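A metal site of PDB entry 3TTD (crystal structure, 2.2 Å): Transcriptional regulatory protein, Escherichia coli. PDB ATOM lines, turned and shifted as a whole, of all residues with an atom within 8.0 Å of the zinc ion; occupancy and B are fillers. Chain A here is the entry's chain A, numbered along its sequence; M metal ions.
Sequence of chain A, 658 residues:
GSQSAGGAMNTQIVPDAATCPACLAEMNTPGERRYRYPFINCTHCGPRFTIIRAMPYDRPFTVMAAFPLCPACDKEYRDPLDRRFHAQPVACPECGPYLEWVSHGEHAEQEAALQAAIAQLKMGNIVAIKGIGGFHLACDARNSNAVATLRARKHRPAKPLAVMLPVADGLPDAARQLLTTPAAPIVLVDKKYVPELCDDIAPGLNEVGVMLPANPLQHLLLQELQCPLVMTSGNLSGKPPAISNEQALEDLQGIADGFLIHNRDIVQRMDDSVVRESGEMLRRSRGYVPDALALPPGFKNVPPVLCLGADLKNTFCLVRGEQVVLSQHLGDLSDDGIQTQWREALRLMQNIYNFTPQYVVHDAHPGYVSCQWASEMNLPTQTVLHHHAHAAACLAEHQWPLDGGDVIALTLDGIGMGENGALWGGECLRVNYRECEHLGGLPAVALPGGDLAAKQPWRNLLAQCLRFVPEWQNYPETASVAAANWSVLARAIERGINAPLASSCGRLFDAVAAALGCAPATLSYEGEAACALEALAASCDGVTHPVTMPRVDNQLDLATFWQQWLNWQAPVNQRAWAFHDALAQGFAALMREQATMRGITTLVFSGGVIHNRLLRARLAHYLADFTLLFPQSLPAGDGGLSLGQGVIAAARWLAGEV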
ATOM      1  N   ALA A  17     -27.307  -3.799 -33.962  1.00  0.00           N
ATOM      2  CA  ALA A  17     -27.707  -5.070 -34.588  1.00  0.00           C
ATOM      3  C   ALA A  17     -29.038  -5.629 -34.111  1.00  0.00           C
ATOM      4  O   ALA A  17     -29.327  -5.607 -32.933  1.00  0.00           O
ATOM      5  CB  ALA A  17     -26.594  -6.164 -34.501  1.00  0.00           C
ATOM      6  N   ALA A  18     -29.846  -6.127 -35.057  1.00  0.00           N
ATOM      7  CA  ALA A  18     -31.137  -6.742 -34.764  1.00  0.00           C
ATOM      8  C   ALA A  18     -30.960  -7.829 -33.714  1.00  0.00           C
ATOM      9  O   ALA A  18     -30.034  -8.610 -33.821  1.00  0.00           O
ATOM     10  CB  ALA A  18     -31.720  -7.362 -36.042  1.00  0.00           C
ATOM     11  N   THR A  19     -31.861  -7.921 -32.739  1.00  0.00           N
ATOM     12  CA  THR A  19     -31.949  -9.086 -31.835  1.00  0.00           C
ATOM     13  C   THR A  19     -31.731 -10.410 -32.606  1.00  0.00           C
ATOM     14  O   THR A  19     -32.390 -10.637 -33.641  1.00  0.00           O
ATOM     15  CB  THR A  19     -33.350  -9.043 -31.145  1.00  0.00           C
ATOM     16  OG1 THR A  19     -33.511  -7.731 -30.580  1.00  0.00           O
ATOM     17  CG2 THR A  19     -33.516 -10.118 -30.022  1.00  0.00           C
ATOM     18  N   CYS A  20     -30.801 -11.279 -32.132  1.00  0.00           N
ATOM     19  CA  CYS A  20     -30.457 -12.537 -32.841  1.00  0.00           C
ATOM     20  C   CYS A  20     -31.442 -13.681 -32.540  1.00  0.00           C
ATOM     21  O   CYS A  20     -32.265 -13.560 -31.638  1.00  0.00           O
ATOM     22  CB  CYS A  20     -29.024 -12.958 -32.504  1.00  0.00           C
ATOM     23  SG  CYS A  20     -28.796 -13.538 -30.760  1.00  0.00           S
ATOM     24  N   PRO A  21     -31.393 -14.782 -33.319  1.00  0.00           N
ATOM     25  CA  PRO A  21     -32.339 -15.897 -33.031  1.00  0.00           C
ATOM     26  C   PRO A  21     -32.265 -16.447 -31.593  1.00  0.00           C
ATOM     27  O   PRO A  21     -33.287 -16.630 -30.949  1.00  0.00           O
ATOM     28  CB  PRO A  21     -31.959 -16.967 -34.057  1.00  0.00           C
ATOM     29  CG  PRO A  21     -31.437 -16.125 -35.243  1.00  0.00           C
ATOM     30  CD  PRO A  21     -30.610 -15.039 -34.538  1.00  0.00           C
ATOM     31  N   ALA A  22     -31.059 -16.620 -31.078  1.00  0.00           N
ATOM     32  CA  ALA A  22     -30.833 -17.100 -29.699  1.00  0.00           C
ATOM     33  C   ALA A  22     -31.382 -16.196 -28.586  1.00  0.00           C
ATOM     34  O   ALA A  22     -31.869 -16.703 -27.587  1.00  0.00           O
ATOM     35  CB  ALA A  22     -29.324 -17.373 -29.493  1.00  0.00           C
ATOM     36  N   CYS A  23     -31.305 -14.880 -28.716  1.00  0.00           N
ATOM     37  CA  CYS A  23     -31.848 -13.959 -27.703  1.00  0.00           C
ATOM     38  C   CYS A  23     -33.372 -13.956 -27.827  1.00  0.00           C
ATOM     39  O   CYS A  23     -34.107 -13.964 -26.832  1.00  0.00           O
ATOM     40  CB  CYS A  23     -31.314 -12.535 -27.868  1.00  0.00           C
ATOM     41  SG  CYS A  23     -29.608 -12.228 -27.225  1.00  0.00           S
ATOM     42  N   LEU A  24     -33.844 -13.961 -29.066  1.00  0.00           N
ATOM     43  CA  LEU A  24     -35.278 -14.106 -29.315  1.00  0.00           C
ATOM     44  C   LEU A  24     -35.889 -15.403 -28.691  1.00  0.00           C
ATOM     45  O   LEU A  24     -36.932 -15.334 -28.042  1.00  0.00           O
ATOM     46  CB  LEU A  24     -35.564 -13.946 -30.805  1.00  0.00           C
ATOM     47  CG  LEU A  24     -37.041 -13.913 -31.123  1.00  0.00           C
ATOM     48  CD1 LEU A  24     -37.710 -12.699 -30.410  1.00  0.00           C
ATOM     49  CD2 LEU A  24     -37.291 -13.962 -32.656  1.00  0.00           C
ATOM     50  N   GLU A  26     -34.499 -17.098 -26.110  1.00  0.00           N
ATOM     51  CA  GLU A  26     -34.378 -16.906 -24.656  1.00  0.00           C
ATOM     52  C   GLU A  26     -35.540 -16.069 -24.140  1.00  0.00           C
ATOM     53  O   GLU A  26     -36.177 -16.437 -23.158  1.00  0.00           O
ATOM     54  CB  GLU A  26     -33.025 -16.269 -24.304  1.00  0.00           C
ATOM     55  CG  GLU A  26     -32.749 -16.023 -22.820  1.00  0.00           C
ATOM     56  CD  GLU A  26     -31.337 -15.437 -22.576  1.00  0.00           C
ATOM     57  OE1 GLU A  26     -30.475 -15.508 -23.499  1.00  0.00           O
ATOM     58  OE2 GLU A  26     -31.118 -14.905 -21.448  1.00  0.00           O
ATOM     59  N   ILE A  40     -33.095  -7.647 -23.560  1.00  0.00           N
ATOM     60  CA  ILE A  40     -32.200  -8.757 -23.793  1.00  0.00           C
ATOM     61  C   ILE A  40     -31.252  -8.439 -24.979  1.00  0.00           C
ATOM     62  O   ILE A  40     -31.690  -7.948 -26.047  1.00  0.00           O
ATOM     63  CB  ILE A  40     -33.013 -10.076 -24.041  1.00  0.00           C
ATOM     64  CG1 ILE A  40     -32.104 -11.309 -24.172  1.00  0.00           C
ATOM     65  CG2 ILE A  40     -33.905  -9.970 -25.268  1.00  0.00           C
ATOM     66  CD1 ILE A  40     -32.912 -12.620 -23.949  1.00  0.00           C
ATOM     67  N   ASN A  41     -29.957  -8.711 -24.780  1.00  0.00           N
ATOM     68  CA  ASN A  41     -28.981  -8.646 -25.878  1.00  0.00           C
ATOM     69  C   ASN A  41     -27.839  -9.590 -25.568  1.00  0.00           C
ATOM     70  O   ASN A  41     -27.737 -10.078 -24.449  1.00  0.00           O
ATOM     71  CB  ASN A  41     -28.460  -7.215 -26.132  1.00  0.00           C
ATOM     72  CG  ASN A  41     -27.854  -6.571 -24.879  1.00  0.00           C
ATOM     73  OD1 ASN A  41     -28.505  -5.776 -24.216  1.00  0.00           O
ATOM     74  ND2 ASN A  41     -26.643  -6.939 -24.527  1.00  0.00           N
ATOM     75  N   CYS A  42     -26.989  -9.860 -26.544  1.00  0.00           N
ATOM     76  CA  CYS A  42     -25.798 -10.649 -26.262  1.00  0.00           C
ATOM     77  C   CYS A  42     -24.604 -10.098 -27.017  1.00  0.00           C
ATOM     78  O   CYS A  42     -24.637  -8.972 -27.536  1.00  0.00           O
ATOM     79  CB  CYS A  42     -26.046 -12.146 -26.566  1.00  0.00           C
ATOM     80  SG  CYS A  42     -26.172 -12.498 -28.304  1.00  0.00           S
ATOM     81  N   THR A  43     -23.531 -10.846 -27.075  1.00  0.00           N
ATOM     82  CA  THR A  43     -22.330 -10.381 -27.767  1.00  0.00           C
ATOM     83  C   THR A  43     -22.549 -10.179 -29.276  1.00  0.00           C
ATOM     84  O   THR A  43     -21.858  -9.375 -29.899  1.00  0.00           O
ATOM     85  CB  THR A  43     -21.085 -11.277 -27.441  1.00  0.00           C
ATOM     86  OG1 THR A  43     -19.884 -10.578 -27.788  1.00  0.00           O
ATOM     87  CG2 THR A  43     -21.143 -12.612 -28.151  1.00  0.00           C
ATOM     88  N   HIS A  44     -23.562 -10.843 -29.827  1.00  0.00           N
ATOM     89  CA  HIS A  44     -23.875 -10.806 -31.263  1.00  0.00           C
ATOM     90  C   HIS A  44     -24.955  -9.815 -31.710  1.00  0.00           C
ATOM     91  O   HIS A  44     -25.193  -9.696 -32.919  1.00  0.00           O
ATOM     92  CB  HIS A  44     -24.220 -12.211 -31.767  1.00  0.00           C
ATOM     93  CG  HIS A  44     -23.113 -13.176 -31.572  1.00  0.00           C
ATOM     94  ND1 HIS A  44     -23.212 -14.272 -30.735  1.00  0.00           N
ATOM     95  CD2 HIS A  44     -21.829 -13.159 -32.030  1.00  0.00           C
ATOM     96  CE1 HIS A  44     -22.060 -14.913 -30.721  1.00  0.00           C
ATOM     97  NE2 HIS A  44     -21.195 -14.256 -31.495  1.00  0.00           N
ATOM     98  N   CYS A  45     -25.618  -9.135 -30.778  1.00  0.00           N
ATOM     99  CA  CYS A  45     -26.773  -8.315 -31.121  1.00  0.00           C
ATOM    100  C   CYS A  45     -27.029  -7.223 -30.081  1.00  0.00           C
ATOM    101  O   CYS A  45     -26.481  -7.266 -28.956  1.00  0.00           O
ATOM    102  CB  CYS A  45     -28.049  -9.168 -31.295  1.00  0.00           C
ATOM    103  SG  CYS A  45     -28.895  -9.624 -29.758  1.00  0.00           S
ATOM    104  N   GLY A  46     -27.870  -6.256 -30.458  1.00  0.00           N
ATOM    105  CA  GLY A  46     -28.266  -5.221 -29.568  1.00  0.00           C
ATOM    106  C   GLY A  46     -27.626  -3.897 -29.968  1.00  0.00           C
ATOM    107  O   GLY A  46     -26.888  -3.827 -30.941  1.00  0.00           O
ATOM    108  N   ARG A  48     -25.312  -0.587 -30.209  1.00  0.00           N
ATOM    109  CA  ARG A  48     -23.851  -0.367 -30.113  1.00  0.00           C
ATOM    110  C   ARG A  48     -23.553   1.144 -30.140  1.00  0.00           C
ATOM    111  O   ARG A  48     -23.487   1.806 -29.103  1.00  0.00           O
ATOM    112  CB  ARG A  48     -23.109  -1.106 -31.261  1.00  0.00           C
ATOM    113  CG  ARG A  48     -23.170  -2.634 -31.217  1.00  0.00           C
ATOM    114  CD  ARG A  48     -22.422  -3.190 -30.001  1.00  0.00           C
ATOM    115  NE  ARG A  48     -22.503  -4.645 -29.977  1.00  0.00           N
ATOM    116  CZ  ARG A  48     -23.420  -5.358 -29.333  1.00  0.00           C
ATOM    117  NH1 ARG A  48     -23.349  -6.665 -29.454  1.00  0.00           N
ATOM    118  NH2 ARG A  48     -24.408  -4.800 -28.604  1.00  0.00           N
ATOM    119  N   ARG A  83     -22.649 -16.905 -24.346  1.00  0.00           N
ATOM    120  CA  ARG A  83     -23.058 -16.010 -25.453  1.00  0.00           C
ATOM    121  C   ARG A  83     -23.027 -14.523 -25.064  1.00  0.00           C
ATOM    122  O   ARG A  83     -22.851 -13.638 -25.914  1.00  0.00           O
ATOM    123  CB  ARG A  83     -24.459 -16.396 -25.935  1.00  0.00           C
ATOM    124  CG  ARG A  83     -24.821 -15.800 -27.303  1.00  0.00           C
ATOM    125  CD  ARG A  83     -26.178 -16.264 -27.792  1.00  0.00           C
ATOM    126  NE  ARG A  83     -27.298 -15.542 -27.215  1.00  0.00           N
ATOM    127  CZ  ARG A  83     -28.080 -15.970 -26.220  1.00  0.00           C
ATOM    128  NH1 ARG A  83     -27.860 -17.125 -25.625  1.00  0.00           N
ATOM    129  NH2 ARG A  83     -29.080 -15.232 -25.791  1.00  0.00           N
ATOM    130  N   ARG A  84     -23.202 -14.272 -23.774  1.00  0.00           N
ATOM    131  CA  ARG A  84     -23.266 -12.913 -23.240  1.00  0.00           C
ATOM    132  C   ARG A  84     -21.916 -12.436 -22.695  1.00  0.00           C
ATOM    133  O   ARG A  84     -21.850 -11.375 -22.034  1.00  0.00           O
ATOM    134  CB  ARG A  84     -24.361 -12.819 -22.171  1.00  0.00           C
ATOM    135  CG  ARG A  84     -25.742 -12.660 -22.773  1.00  0.00           C
ATOM    136  CD  ARG A  84     -26.839 -13.313 -21.950  1.00  0.00           C
ATOM    137  NE  ARG A  84     -27.149 -14.678 -22.382  1.00  0.00           N
ATOM    138  CZ  ARG A  84     -26.850 -15.797 -21.701  1.00  0.00           C
ATOM    139  NH1 ARG A  84     -26.211 -15.748 -20.530  1.00  0.00           N
ATOM    140  NH2 ARG A  84     -27.184 -16.984 -22.178  1.00  0.00           N
ATOM    141  N   ALA A  87     -20.857  -8.891 -23.035  1.00  0.00           N
ATOM    142  CA  ALA A  87     -21.957  -8.184 -23.677  1.00  0.00           C
ATOM    143  C   ALA A  87     -22.127  -6.889 -22.872  1.00  0.00           C
ATOM    144  O   ALA A  87     -22.771  -6.878 -21.835  1.00  0.00           O
ATOM    145  CB  ALA A  87     -23.258  -9.031 -23.701  1.00  0.00           C
HETATM  146 ZN    ZN M   1     -28.340 -11.898 -29.080  1.00  0.00          ZN
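The zinc ion is bound by the side-chain sulfur of Cys 23, the side-chain sulfur of Cys 42, the side-chain sulfur of Cys 20 and the side-chain sulfur of Cys 45.
SG of Cys 23 sits close to NH2 of Arg 83 (3.4 Å).
The side-chain sulfur of Cys 42 lies close to the backbone NH of His 44 (3.4 Å).
The backbone carbonyl oxygen (O) of Cys 45 lies within hydrogen-bond range of the guanidinium group (NH1) of Arg 48, at 3.2 Å.
The side-chain sulfur (SG) of Cys 42 sits close to the guanidinium group (NE) of Arg 83, 3.4 Å away.
O of Cys 42 sits at hydrogen-bond distance from NH1 of Arg 48.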
